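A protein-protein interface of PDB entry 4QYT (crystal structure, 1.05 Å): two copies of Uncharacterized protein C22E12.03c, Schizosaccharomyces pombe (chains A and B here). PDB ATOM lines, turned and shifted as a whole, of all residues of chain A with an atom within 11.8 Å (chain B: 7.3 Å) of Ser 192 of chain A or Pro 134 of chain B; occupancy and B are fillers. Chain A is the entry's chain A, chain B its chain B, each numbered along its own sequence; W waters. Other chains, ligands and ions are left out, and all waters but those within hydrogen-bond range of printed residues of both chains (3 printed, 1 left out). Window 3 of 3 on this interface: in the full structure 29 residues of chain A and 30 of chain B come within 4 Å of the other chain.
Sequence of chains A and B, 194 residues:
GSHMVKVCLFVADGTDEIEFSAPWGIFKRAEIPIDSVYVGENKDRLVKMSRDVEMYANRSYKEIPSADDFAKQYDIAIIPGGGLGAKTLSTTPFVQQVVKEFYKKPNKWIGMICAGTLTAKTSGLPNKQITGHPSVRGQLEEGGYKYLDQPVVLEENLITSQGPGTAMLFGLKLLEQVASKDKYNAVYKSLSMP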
ATOM      1  N   GLY A  25     -26.356  28.283  13.327  1.00  0.00           N
ATOM      2  CA  GLY A  25     -24.994  27.829  13.194  1.00  0.00           C
ATOM      3  C   GLY A  25     -24.199  28.606  12.165  1.00  0.00           C
ATOM      4  O   GLY A  25     -22.981  28.770  12.310  1.00  0.00           O
ATOM      5  N   ILE A  26     -24.871  29.059  11.127  1.00  0.00           N
ATOM      6  CA  ILE A  26     -24.196  29.846  10.065  1.00  0.00           C
ATOM      7  C   ILE A  26     -23.779  31.208  10.597  1.00  0.00           C
ATOM      8  O   ILE A  26     -22.634  31.627  10.409  1.00  0.00           O
ATOM      9  CB  ILE A  26     -25.092  29.904   8.819  1.00  0.00           C
ATOM     10  CG1 ILE A  26     -25.142  28.519   8.155  1.00  0.00           C
ATOM     11  CG2 ILE A  26     -24.606  30.953   7.814  1.00  0.00           C
ATOM     12  CD1 ILE A  26     -26.256  28.352   7.143  1.00  0.00           C
ATOM     13  N   ARG A  29     -20.913  30.848  13.060  1.00  0.00           N
ATOM     14  CA  ARG A  29     -19.638  30.657  12.370  1.00  0.00           C
ATOM     15  C   ARG A  29     -19.103  31.961  11.800  1.00  0.00           C
ATOM     16  O   ARG A  29     -17.885  32.149  11.682  1.00  0.00           O
ATOM     17  CB  ARG A  29     -19.797  29.631  11.266  1.00  0.00           C
ATOM     18  CG  ARG A  29     -19.849  28.188  11.792  1.00  0.00           C
ATOM     19  CD  ARG A  29     -20.328  27.248  10.716  1.00  0.00           C
ATOM     20  NE  ARG A  29     -20.264  25.837  11.081  1.00  0.00           N
ATOM     21  CZ  ARG A  29     -21.098  25.252  11.917  1.00  0.00           C
ATOM     22  NH1 ARG A  29     -22.140  25.906  12.422  1.00  0.00           N
ATOM     23  NH2 ARG A  29     -20.970  23.954  12.164  1.00  0.00           N
ATOM     24  N   GLY A 165     -34.971  20.882   4.202  1.00  0.00           N
ATOM     25  CA  GLY A 165     -33.896  20.629   3.244  1.00  0.00           C
ATOM     26  C   GLY A 165     -33.233  21.858   2.678  1.00  0.00           C
ATOM     27  O   GLY A 165     -32.133  21.755   2.168  1.00  0.00           O
ATOM     28  N   MET A 168     -30.125  25.285   5.131  1.00  0.00           N
ATOM     29  CA  MET A 168     -28.760  25.738   4.951  1.00  0.00           C
ATOM     30  C   MET A 168     -28.638  26.786   3.838  1.00  0.00           C
ATOM     31  O   MET A 168     -28.017  27.832   4.011  1.00  0.00           O
ATOM     32  CB  MET A 168     -27.805  24.564   4.686  1.00  0.00           C
ATOM     33  CG  MET A 168     -27.626  23.629   5.887  1.00  0.00           C
ATOM     34  SD  MET A 168     -26.825  24.390   7.309  1.00  0.00           S
ATOM     35  CE  MET A 168     -25.173  24.516   6.662  1.00  0.00           C
ATOM     36  N   LEU A 169     -29.277  26.523   2.700  1.00  0.00           N
ATOM     37  CA  LEU A 169     -29.302  27.520   1.620  1.00  0.00           C
ATOM     38  C   LEU A 169     -29.933  28.830   2.052  1.00  0.00           C
ATOM     39  O   LEU A 169     -29.469  29.928   1.673  1.00  0.00           O
ATOM     40  CB  LEU A 169     -30.038  26.967   0.410  1.00  0.00           C
ATOM     41  CG  LEU A 169     -29.307  25.859  -0.347  1.00  0.00           C
ATOM     42  CD1 LEU A 169     -30.279  25.184  -1.274  1.00  0.00           C
ATOM     43  CD2 LEU A 169     -28.097  26.393  -1.105  1.00  0.00           C
ATOM     44  N   LEU A 172     -27.515  30.702   4.387  1.00  0.00           N
ATOM     45  CA  LEU A 172     -26.459  31.251   3.562  1.00  0.00           C
ATOM     46  C   LEU A 172     -26.940  32.488   2.792  1.00  0.00           C
ATOM     47  O   LEU A 172     -26.161  33.470   2.658  1.00  0.00           O
ATOM     48  CB  LEU A 172     -25.904  30.201   2.602  1.00  0.00           C
ATOM     49  CG  LEU A 172     -24.959  29.202   3.218  1.00  0.00           C
ATOM     50  CD1 LEU A 172     -24.771  28.012   2.273  1.00  0.00           C
ATOM     51  CD2 LEU A 172     -23.631  29.833   3.596  1.00  0.00           C
ATOM     52  N   TYR A 184     -18.106  35.527   3.608  1.00  0.00           N
ATOM     53  CA  TYR A 184     -19.080  34.587   3.081  1.00  0.00           C
ATOM     54  C   TYR A 184     -18.397  33.333   2.565  1.00  0.00           C
ATOM     55  O   TYR A 184     -18.764  32.193   2.895  1.00  0.00           O
ATOM     56  CB  TYR A 184     -19.931  35.232   1.999  1.00  0.00           C
ATOM     57  CG  TYR A 184     -20.926  34.260   1.420  1.00  0.00           C
ATOM     58  CD1 TYR A 184     -22.136  34.012   2.057  1.00  0.00           C
ATOM     59  CD2 TYR A 184     -20.656  33.524   0.300  1.00  0.00           C
ATOM     60  CE1 TYR A 184     -23.063  33.093   1.570  1.00  0.00           C
ATOM     61  CE2 TYR A 184     -21.533  32.563  -0.156  1.00  0.00           C
ATOM     62  CZ  TYR A 184     -22.762  32.385   0.458  1.00  0.00           C
ATOM     63  OH  TYR A 184     -23.662  31.442  -0.026  1.00  0.00           O
ATOM     64  N   ASN A 185     -17.366  33.530   1.766  1.00  0.00           N
ATOM     65  CA  ASN A 185     -16.730  32.387   1.120  1.00  0.00           C
ATOM     66  C   ASN A 185     -16.073  31.459   2.141  1.00  0.00           C
ATOM     67  O   ASN A 185     -16.087  30.230   2.002  1.00  0.00           O
ATOM     68  CB  ASN A 185     -15.690  32.847   0.091  1.00  0.00           C
ATOM     69  CG  ASN A 185     -16.316  33.381  -1.183  1.00  0.00           C
ATOM     70  OD1 ASN A 185     -17.500  33.174  -1.473  1.00  0.00           O
ATOM     71  ND2 ASN A 185     -15.501  34.075  -1.970  1.00  0.00           N
ATOM     72  N   ALA A 186     -15.469  32.044   3.162  1.00  0.00           N
ATOM     73  CA  ALA A 186     -14.794  31.272   4.185  1.00  0.00           C
ATOM     74  C   ALA A 186     -15.864  30.458   4.930  1.00  0.00           C
ATOM     75  O   ALA A 186     -15.657  29.264   5.239  1.00  0.00           O
ATOM     76  CB  ALA A 186     -14.086  32.175   5.158  1.00  0.00           C
ATOM     77  N   VAL A 187     -16.955  31.094   5.374  1.00  0.00           N
ATOM     78  CA  VAL A 187     -18.005  30.339   6.094  1.00  0.00           C
ATOM     79  C   VAL A 187     -18.521  29.238   5.193  1.00  0.00           C
ATOM     80  O   VAL A 187     -18.673  28.080   5.633  1.00  0.00           O
ATOM     81  CB  VAL A 187     -19.124  31.262   6.581  1.00  0.00           C
ATOM     82  CG1 VAL A 187     -20.275  30.453   7.121  1.00  0.00           C
ATOM     83  CG2 VAL A 187     -18.578  32.212   7.648  1.00  0.00           C
ATOM     84  N   TYR A 188     -18.863  29.593   3.961  1.00  0.00           N
ATOM     85  CA  TYR A 188     -19.387  28.624   3.021  1.00  0.00           C
ATOM     86  C   TYR A 188     -18.492  27.401   2.931  1.00  0.00           C
ATOM     87  O   TYR A 188     -18.946  26.242   2.978  1.00  0.00           O
ATOM     88  CB  TYR A 188     -19.594  29.263   1.630  1.00  0.00           C
ATOM     89  CG  TYR A 188     -20.227  28.354   0.598  1.00  0.00           C
ATOM     90  CD1 TYR A 188     -19.470  27.448  -0.129  1.00  0.00           C
ATOM     91  CD2 TYR A 188     -21.602  28.425   0.335  1.00  0.00           C
ATOM     92  CE1 TYR A 188     -20.073  26.571  -1.018  1.00  0.00           C
ATOM     93  CE2 TYR A 188     -22.193  27.607  -0.608  1.00  0.00           C
ATOM     94  CZ  TYR A 188     -21.423  26.687  -1.286  1.00  0.00           C
ATOM     95  OH  TYR A 188     -21.999  25.853  -2.222  1.00  0.00           O
ATOM     96  N   LYS A 189     -17.210  27.633   2.695  1.00  0.00           N
ATOM     97  CA  LYS A 189     -16.256  26.536   2.551  1.00  0.00           C
ATOM     98  C   LYS A 189     -16.239  25.606   3.753  1.00  0.00           C
ATOM     99  O   LYS A 189     -16.121  24.396   3.610  1.00  0.00           O
ATOM    100  CB  LYS A 189     -14.855  27.101   2.282  1.00  0.00           C
ATOM    101  CG  LYS A 189     -13.776  26.061   2.063  1.00  0.00           C
ATOM    102  CD  LYS A 189     -12.392  26.661   1.882  1.00  0.00           C
ATOM    103  CE  LYS A 189     -11.338  25.649   1.454  1.00  0.00           C
ATOM    104  NZ  LYS A 189      -9.988  26.258   1.612  1.00  0.00           N
ATOM    105  N   SER A 190     -16.378  26.168   4.938  1.00  0.00           N
ATOM    106  CA  SER A 190     -16.342  25.402   6.178  1.00  0.00           C
ATOM    107  C   SER A 190     -17.528  24.448   6.344  1.00  0.00           C
ATOM    108  O   SER A 190     -17.458  23.548   7.177  1.00  0.00           O
ATOM    109  CB  SER A 190     -16.261  26.317   7.403  1.00  0.00           C
ATOM    110  OG  SER A 190     -17.521  26.883   7.733  1.00  0.00           O
ATOM    111  N   LEU A 191     -18.602  24.647   5.580  1.00  0.00           N
ATOM    112  CA  LEU A 191     -19.795  23.870   5.781  1.00  0.00           C
ATOM    113  C   LEU A 191     -19.813  22.551   5.056  1.00  0.00           C
ATOM    114  O   LEU A 191     -20.652  21.703   5.374  1.00  0.00           O
ATOM    115  CB  LEU A 191     -20.995  24.676   5.373  1.00  0.00           C
ATOM    116  CG  LEU A 191     -21.192  25.993   6.083  1.00  0.00           C
ATOM    117  CD1 LEU A 191     -22.337  26.798   5.470  1.00  0.00           C
ATOM    118  CD2 LEU A 191     -21.419  25.817   7.568  1.00  0.00           C
ATOM    119  N   SER A 192     -18.968  22.356   4.056  1.00  0.00           N
ATOM    120  CA  SER A 192     -19.096  21.172   3.182  1.00  0.00           C
ATOM    121  C   SER A 192     -20.433  21.081   2.460  1.00  0.00           C
ATOM    122  O   SER A 192     -21.059  20.023   2.443  1.00  0.00           O
ATOM    123  CB  SER A 192     -18.792  19.865   3.902  1.00  0.00           C
ATOM    124  OG  SER A 192     -17.474  19.871   4.351  1.00  0.00           O
ATOM    125  N   MET A 193     -20.824  22.156   1.796  1.00  0.00           N
ATOM    126  CA  MET A 193     -22.032  22.138   1.008  1.00  0.00           C
ATOM    127  C   MET A 193     -21.854  21.168  -0.134  1.00  0.00           C
ATOM    128  O   MET A 193     -20.782  21.080  -0.753  1.00  0.00           O
ATOM    129  CB  MET A 193     -22.323  23.518   0.482  1.00  0.00           C
ATOM    130  CG  MET A 193     -22.583  24.532   1.577  1.00  0.00           C
ATOM    131  SD  MET A 193     -24.050  24.180   2.578  1.00  0.00           S
ATOM    132  CE  MET A 193     -25.341  24.474   1.351  1.00  0.00           C
ATOM    133  N   PRO A 194     -22.901  20.390  -0.403  1.00  0.00           N
ATOM    134  CA  PRO A 194     -22.778  19.356  -1.408  1.00  0.00           C
ATOM    135  C   PRO A 194     -22.816  19.959  -2.784  1.00  0.00           C
ATOM    136  O   PRO A 194     -23.260  21.096  -2.998  1.00  0.00           O
ATOM    137  CB  PRO A 194     -23.987  18.473  -1.155  1.00  0.00           C
ATOM    138  CG  PRO A 194     -24.957  19.299  -0.401  1.00  0.00           C
ATOM    139  CD  PRO A 194     -24.156  20.307   0.356  1.00  0.00           C
ATOM    140  OXT PRO A 194     -22.221  19.360  -3.700  1.00  0.00           O
ATOM    141  N   CSD B 114     -18.781  14.691  10.202  1.00  0.00           N
ATOM    142  CA  CSD B 114     -17.803  15.788  10.417  1.00  0.00           C
ATOM    143  CB  CSD B 114     -18.525  17.039  10.980  1.00  0.00           C
ATOM    144  SG  CSD B 114     -17.731  18.554  11.301  1.00  0.00           S
ATOM    145  C   CSD B 114     -16.651  15.205  11.210  1.00  0.00           C
ATOM    146  O   CSD B 114     -16.120  14.150  10.860  1.00  0.00           O
ATOM    147  OD1 CSD B 114     -18.805  19.558  11.199  1.00  0.00           O
ATOM    148  OD2 CSD B 114     -17.403  18.362  12.803  1.00  0.00           O
ATOM    149  N   THR B 131     -15.946   8.843   4.486  1.00  0.00           N
ATOM    150  CA  THR B 131     -15.752  10.284   4.383  1.00  0.00           C
ATOM    151  C   THR B 131     -15.879  10.935   5.752  1.00  0.00           C
ATOM    152  O   THR B 131     -16.084  10.252   6.755  1.00  0.00           O
ATOM    153  CB  THR B 131     -16.699  10.953   3.344  1.00  0.00           C
ATOM    154  OG1 THR B 131     -16.204  12.250   2.998  1.00  0.00           O
ATOM    155  CG2 THR B 131     -18.132  11.054   3.844  1.00  0.00           C
ATOM    156  N   GLY B 132     -15.689  12.255   5.775  1.00  0.00           N
ATOM    157  CA  GLY B 132     -15.752  13.043   6.993  1.00  0.00           C
ATOM    158  C   GLY B 132     -15.410  14.468   6.609  1.00  0.00           C
ATOM    159  O   GLY B 132     -15.304  14.804   5.427  1.00  0.00           O
ATOM    160  N   HIS B 133     -15.325  15.351   7.592  1.00  0.00           N
ATOM    161  CA  HIS B 133     -15.071  16.750   7.273  1.00  0.00           C
ATOM    162  C   HIS B 133     -13.692  16.855   6.654  1.00  0.00           C
ATOM    163  O   HIS B 133     -12.769  16.146   7.056  1.00  0.00           O
ATOM    164  CB  HIS B 133     -15.161  17.629   8.520  1.00  0.00           C
ATOM    165  CG  HIS B 133     -15.257  19.084   8.205  1.00  0.00           C
ATOM    166  ND1 HIS B 133     -14.160  19.914   8.164  1.00  0.00           N
ATOM    167  CD2 HIS B 133     -16.320  19.842   7.847  1.00  0.00           C
ATOM    168  CE1 HIS B 133     -14.555  21.134   7.840  1.00  0.00           C
ATOM    169  NE2 HIS B 133     -15.853  21.105   7.595  1.00  0.00           N
ATOM    170  N   PRO B 134     -13.527  17.743   5.675  1.00  0.00           N
ATOM    171  CA  PRO B 134     -12.214  17.814   5.034  1.00  0.00           C
ATOM    172  C   PRO B 134     -11.078  18.152   6.001  1.00  0.00           C
ATOM    173  O   PRO B 134      -9.956  17.701   5.800  1.00  0.00           O
ATOM    174  CB  PRO B 134     -12.399  18.906   3.984  1.00  0.00           C
ATOM    175  CG  PRO B 134     -13.847  18.817   3.612  1.00  0.00           C
ATOM    176  CD  PRO B 134     -14.545  18.493   4.910  1.00  0.00           C
ATOM    177  N   SER B 135     -11.399  18.761   7.135  1.00  0.00           N
ATOM    178  CA  SER B 135     -10.380  19.017   8.156  1.00  0.00           C
ATOM    179  C   SER B 135      -9.848  17.785   8.893  1.00  0.00           C
ATOM    180  O   SER B 135      -8.782  17.860   9.502  1.00  0.00           O
ATOM    181  CB  SER B 135     -10.909  19.995   9.196  1.00  0.00           C
ATOM    182  OG  SER B 135     -11.923  19.397   9.983  1.00  0.00           O
ATOM    183  N   VAL B 136     -10.559  16.657   8.796  1.00  0.00           N
ATOM    184  CA  VAL B 136     -10.085  15.394   9.363  1.00  0.00           C
ATOM    185  C   VAL B 136      -9.729  14.358   8.309  1.00  0.00           C
ATOM    186  O   VAL B 136      -9.387  13.231   8.655  1.00  0.00           O
ATOM    187  CB  VAL B 136     -11.093  14.783  10.365  1.00  0.00           C
ATOM    188  CG1 VAL B 136     -11.399  15.765  11.484  1.00  0.00           C
ATOM    189  CG2 VAL B 136     -12.362  14.292   9.690  1.00  0.00           C
ATOM    190  N   ARG B 137      -9.619  14.788   7.052  1.00  0.00           N
ATOM    191  CA  ARG B 137      -9.239  13.886   5.987  1.00  0.00           C
ATOM    192  C   ARG B 137      -7.874  13.255   6.244  1.00  0.00           C
ATOM    193  O   ARG B 137      -7.706  12.030   6.080  1.00  0.00           O
ATOM    194  CB  ARG B 137      -9.229  14.597   4.639  1.00  0.00           C
ATOM    195  CG  ARG B 137      -8.749  13.698   3.508  1.00  0.00           C
ATOM    196  CD  ARG B 137      -8.868  14.387   2.165  1.00  0.00           C
ATOM    197  NE  ARG B 137      -8.597  13.467   1.065  1.00  0.00           N
ATOM    198  CZ  ARG B 137      -9.038  13.654  -0.177  1.00  0.00           C
ATOM    199  NH1 ARG B 137      -9.830  14.684  -0.462  1.00  0.00           N
ATOM    200  NH2 ARG B 137      -8.816  12.740  -1.108  1.00  0.00           N
ATOM    201  N   GLY B 138      -6.888  14.072   6.593  1.00  0.00           N
ATOM    202  CA  GLY B 138      -5.533  13.561   6.792  1.00  0.00           C
ATOM    203  C   GLY B 138      -5.465  12.536   7.903  1.00  0.00           C
ATOM    204  O   GLY B 138      -4.820  11.492   7.787  1.00  0.00           O
ATOM    205  N   GLN B 139      -6.188  12.814   8.983  1.00  0.00           N
ATOM    206  CA  GLN B 139      -6.273  11.855  10.078  1.00  0.00           C
ATOM    207  C   GLN B 139      -6.950  10.533   9.694  1.00  0.00           C
ATOM    208  O   GLN B 139      -6.495   9.455  10.061  1.00  0.00           O
ATOM    209  CB  GLN B 139      -6.999  12.476  11.267  1.00  0.00           C
ATOM    210  CG  GLN B 139      -6.223  13.535  12.029  1.00  0.00           C
ATOM    211  CD  GLN B 139      -7.002  14.018  13.235  1.00  0.00           C
ATOM    212  OE1 GLN B 139      -7.480  15.150  13.252  1.00  0.00           O
ATOM    213  NE2 GLN B 139      -7.214  13.132  14.209  1.00  0.00           N
ATOM    214  N   TYR B 147     -10.357   8.023   1.682  1.00  0.00           N
ATOM    215  CA  TYR B 147     -11.304   9.122   1.822  1.00  0.00           C
ATOM    216  C   TYR B 147     -11.969   9.430   0.497  1.00  0.00           C
ATOM    217  O   TYR B 147     -11.296   9.647  -0.508  1.00  0.00           O
ATOM    218  CB  TYR B 147     -10.577  10.369   2.321  1.00  0.00           C
ATOM    219  CG  TYR B 147     -11.461  11.565   2.557  1.00  0.00           C
ATOM    220  CD1 TYR B 147     -11.757  12.453   1.528  1.00  0.00           C
ATOM    221  CD2 TYR B 147     -11.918  11.874   3.843  1.00  0.00           C
ATOM    222  CE1 TYR B 147     -12.573  13.548   1.749  1.00  0.00           C
ATOM    223  CE2 TYR B 147     -12.681  13.006   4.079  1.00  0.00           C
ATOM    224  CZ  TYR B 147     -13.042  13.819   3.014  1.00  0.00           C
ATOM    225  OH  TYR B 147     -13.852  14.913   3.217  1.00  0.00           O
ATOM    226  N   ASP B 149     -14.375  12.117  -1.412  1.00  0.00           N
ATOM    227  CA  ASP B 149     -14.827  13.492  -1.302  1.00  0.00           C
ATOM    228  C   ASP B 149     -16.232  13.577  -1.879  1.00  0.00           C
ATOM    229  O   ASP B 149     -16.433  13.888  -3.060  1.00  0.00           O
ATOM    230  CB  ASP B 149     -13.887  14.438  -2.042  1.00  0.00           C
ATOM    231  CG  ASP B 149     -14.266  15.902  -1.891  1.00  0.00           C
ATOM    232  OD1 ASP B 149     -15.126  16.236  -1.051  1.00  0.00           O
ATOM    233  OD2 ASP B 149     -13.776  16.696  -2.716  1.00  0.00           O
ATOM    234  N   PRO B 151     -20.755  13.673  -0.309  1.00  0.00           N
ATOM    235  CA  PRO B 151     -21.479  14.029   0.908  1.00  0.00           C
ATOM    236  C   PRO B 151     -21.663  12.887   1.890  1.00  0.00           C
ATOM    237  O   PRO B 151     -21.606  13.142   3.084  1.00  0.00           O
ATOM    238  CB  PRO B 151     -22.824  14.520   0.374  1.00  0.00           C
ATOM    239  CG  PRO B 151     -22.484  15.130  -0.936  1.00  0.00           C
ATOM    240  CD  PRO B 151     -21.406  14.248  -1.501  1.00  0.00           C
ATOM    241  N   SER B 161     -20.171  11.058   6.894  1.00  0.00           N
ATOM    242  CA  SER B 161     -20.546  12.258   6.141  1.00  0.00           C
ATOM    243  C   SER B 161     -19.687  13.446   6.546  1.00  0.00           C
ATOM    244  O   SER B 161     -18.985  13.388   7.539  1.00  0.00           O
ATOM    245  CB  SER B 161     -22.027  12.490   6.340  1.00  0.00           C
ATOM    246  OG  SER B 161     -22.562  13.486   5.517  1.00  0.00           O
ATOM    247  N   GLN B 162     -19.690  14.496   5.725  1.00  0.00           N
ATOM    248  CA  GLN B 162     -18.658  15.542   5.795  1.00  0.00           C
ATOM    249  C   GLN B 162     -18.873  16.699   6.779  1.00  0.00           C
ATOM    250  O   GLN B 162     -17.914  17.139   7.423  1.00  0.00           O
ATOM    251  CB  GLN B 162     -18.415  16.135   4.414  1.00  0.00           C
ATOM    252  CG  GLN B 162     -17.840  15.139   3.446  1.00  0.00           C
ATOM    253  CD  GLN B 162     -17.446  15.787   2.123  1.00  0.00           C
ATOM    254  OE1 GLN B 162     -18.297  16.345   1.429  1.00  0.00           O
ATOM    255  NE2 GLN B 162     -16.213  15.581   1.707  1.00  0.00           N
ATOM    256  N   GLY B 163     -20.072  17.264   6.853  1.00  0.00           N
ATOM    257  CA  GLY B 163     -20.192  18.523   7.583  1.00  0.00           C
ATOM    258  C   GLY B 163     -21.619  18.998   7.708  1.00  0.00           C
ATOM    259  O   GLY B 163     -22.565  18.289   7.356  1.00  0.00           O
ATOM    260  N   PRO B 164     -21.808  20.197   8.265  1.00  0.00           N
ATOM    261  CA  PRO B 164     -23.168  20.682   8.453  1.00  0.00           C
ATOM    262  C   PRO B 164     -23.955  20.677   7.147  1.00  0.00           C
ATOM    263  O   PRO B 164     -25.154  20.367   7.169  1.00  0.00           O
ATOM    264  CB  PRO B 164     -22.999  22.068   9.063  1.00  0.00           C
ATOM    265  CG  PRO B 164     -21.590  22.213   9.303  1.00  0.00           C
ATOM    266  CD  PRO B 164     -20.795  21.150   8.764  1.00  0.00           C
ATOM    267  N   GLY B 165     -23.309  21.013   6.028  1.00  0.00           N
ATOM    268  CA  GLY B 165     -23.992  21.025   4.762  1.00  0.00           C
ATOM    269  C   GLY B 165     -24.483  19.677   4.248  1.00  0.00           C
ATOM    270  O   GLY B 165     -25.349  19.655   3.393  1.00  0.00           O
ATOM    271  N   THR B 166     -23.965  18.604   4.824  1.00  0.00           N
ATOM    272  CA  THR B 166     -24.345  17.253   4.400  1.00  0.00           C
ATOM    273  C   THR B 166     -25.183  16.551   5.448  1.00  0.00           C
ATOM    274  O   THR B 166     -25.485  15.371   5.269  1.00  0.00           O
ATOM    275  CB  THR B 166     -23.106  16.414   4.032  1.00  0.00           C
ATOM    276  OG1 THR B 166     -22.303  16.161   5.178  1.00  0.00           O
ATOM    277  CG2 THR B 166     -22.257  17.118   3.003  1.00  0.00           C
ATOM    278  N   ALA B 167     -25.593  17.243   6.502  1.00  0.00           N
ATOM    279  CA  ALA B 167     -26.295  16.587   7.601  1.00  0.00           C
ATOM    280  C   ALA B 167     -27.635  16.007   7.167  1.00  0.00           C
ATOM    281  O   ALA B 167     -28.028  14.928   7.665  1.00  0.00           O
ATOM    282  CB  ALA B 167     -26.416  17.511   8.794  1.00  0.00           C
ATOM    283  N   LEU B 169     -28.451  14.966   4.057  1.00  0.00           N
ATOM    284  CA  LEU B 169     -28.155  13.783   3.252  1.00  0.00           C
ATOM    285  C   LEU B 169     -27.716  12.619   4.146  1.00  0.00           C
ATOM    286  O   LEU B 169     -28.072  11.463   3.894  1.00  0.00           O
ATOM    287  CB  LEU B 169     -27.045  14.104   2.252  1.00  0.00           C
ATOM    288  CG  LEU B 169     -27.455  15.097   1.174  1.00  0.00           C
ATOM    289  CD1 LEU B 169     -26.234  15.586   0.448  1.00  0.00           C
ATOM    290  CD2 LEU B 169     -28.434  14.440   0.217  1.00  0.00           C
HETATM  291  O   HOH W   1     -26.940  21.886   2.841  1.00  0.00           O
HETATM  292  O   HOH W   2     -15.606  21.861   4.692  1.00  0.00           O
HETATM  293  O   HOH W   3     -18.664  22.271  11.469  1.00  0.00           O
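Among the printed residues, merely in contact across the chains: Ser 192 of chain A with Thr 166 of chain B, Ser 192 of chain A with Pro 134 of chain B, Pro 194 of chain A with Gly 165 of chain B, Arg 29 of chain A with Pro 164 of chain B, Pro 194 of chain A with Pro 151 of chain B, Ser 192 of chain A with His 133 of chain B, Leu 191 of chain A with Gly 163 of chain B, Ser 192 of chain A with Gln 162 of chain B, Met 193 of chain A with Gly 165 of chain B, Ser 192 of chain A with Gly 165 of chain B and Pro 194 of chain A with Leu 169 of chain B.
Of the 21 printed residues of chain B, 9 touch a printed residue of chain A. Hydrophobic or aromatic side chains of chain B within 4 Å of the printed part of chain A: His 133, Pro 134, Pro 151, Pro 164 and Leu 169. Of the 18 printed residues of chain A, 6 touch a printed residue of chain B. Printed residues of chain A that touch a printed residue of chain B: Arg 29, Ser 190, Leu 191, Ser 192, Met 193 and Pro 194. Hydrophobic or aromatic side chains of chain A that line the printed part of chain B: Met 193 and Pro 194. Among the printed residues, no Asp or Glu carboxylate lies within 4 Å of a Lys or Arg side-chain nitrogen of the other chain.
Printed residues of chain B within 4 Å of Ser 192 of chain A: His 133, Pro 134, Gln 162, Gly 165 and Thr 166. Of the printed residues of chain A, Pro 134 of chain B touches Ser 192. Of chain A, only Ser 192 comes within 4 Å of Gln 162 of chain B. Of chain A, only Leu 191 (3.7 Å) comes within 4 Å of Gly 163 of chain B. Pro 164 of chain B touches just these residues of chain A: Arg 29 (3.4 Å) and Leu 191 (3.4 Å). Of the printed residues of chain B, Arg 29 of chain A touches Pro 164 (3.4 Å). Printed residues of chain A within 4 Å of Leu 169 of chain B: Pro 194 (3.99 Å). Of the printed residues of chain B, Ser 190 of chain A touches His 133. Of the printed residues of chain B, Leu 191 of chain A touches Gly 163 (3.7 Å), Pro 164 (3.4 Å) and Gly 165 (2.8 Å). Lys 189 of chain A touches none of the printed residues of chain B. The nearest printed residue of chain B that does not touch Ser 190 of chain A is Pro 164 of chain B (4.4 Å).
O of Gly 25 of chain A lies within hydrogen-bond range of NH1 of Arg 29 of chain A, 3.0 Å away. A ring nitrogen (ND1) of His 133 of chain B is in hydrogen-bond range of the side-chain hydroxyl of Ser 135 of chain B (2.9 Å). The backbone carbonyl oxygen (O) of Gln 162 of chain B sits close to the backbone NH (N) of His 133 of chain B. OG of Ser 161 of chain B is in hydrogen-bond range of OG1 of Thr 166 of chain B, 2.7 Å away. The side-chain hydroxyl of Thr 166 of chain B is in hydrogen-bond range of the backbone NH of Gln 162 of chain B (3.1 Å). OG1 of Thr 166 of chain B is in hydrogen-bond range of N of Gly 163 of chain B (3.0 Å).
Water W3 lies within hydrogen-bond range of OD1 of CSD 114 of chain B (2.7 Å) and the guanidinium group of Arg 29 of chain A (2.9 Å). Water W2 lies within hydrogen-bond range of the side-chain hydroxyl of Ser 192 of chain A (2.8 Å), the backbone carbonyl oxygen of Lys 189 of chain A (2.8 Å) and a ring nitrogen (NE2) of His 133 of chain B (3.0 Å). Water W1 bridges O of Gly 165 of chain B (2.8 Å) and SD of Met 193 of chain A (3.7 Å).
Positions printed for both chains: 165 and 169. Of the 14 pairs that touch across the chains among the printed residues, none has its exchanged pair printed and touching as well.
A ring nitrogen (NE2) of His 133 of chain B is in hydrogen-bond range of the backbone carbonyl oxygen (O) of Ser 190 of chain A (3.0 Å). O of Leu 191 of chain A sits at hydrogen-bond distance from N of Gly 165 of chain B, 2.8 Å away. The backbone carbonyl oxygen of Leu 191 of chain A sits close to the backbone nitrogen of Pro 164 of chain B, at 3.5 Å.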
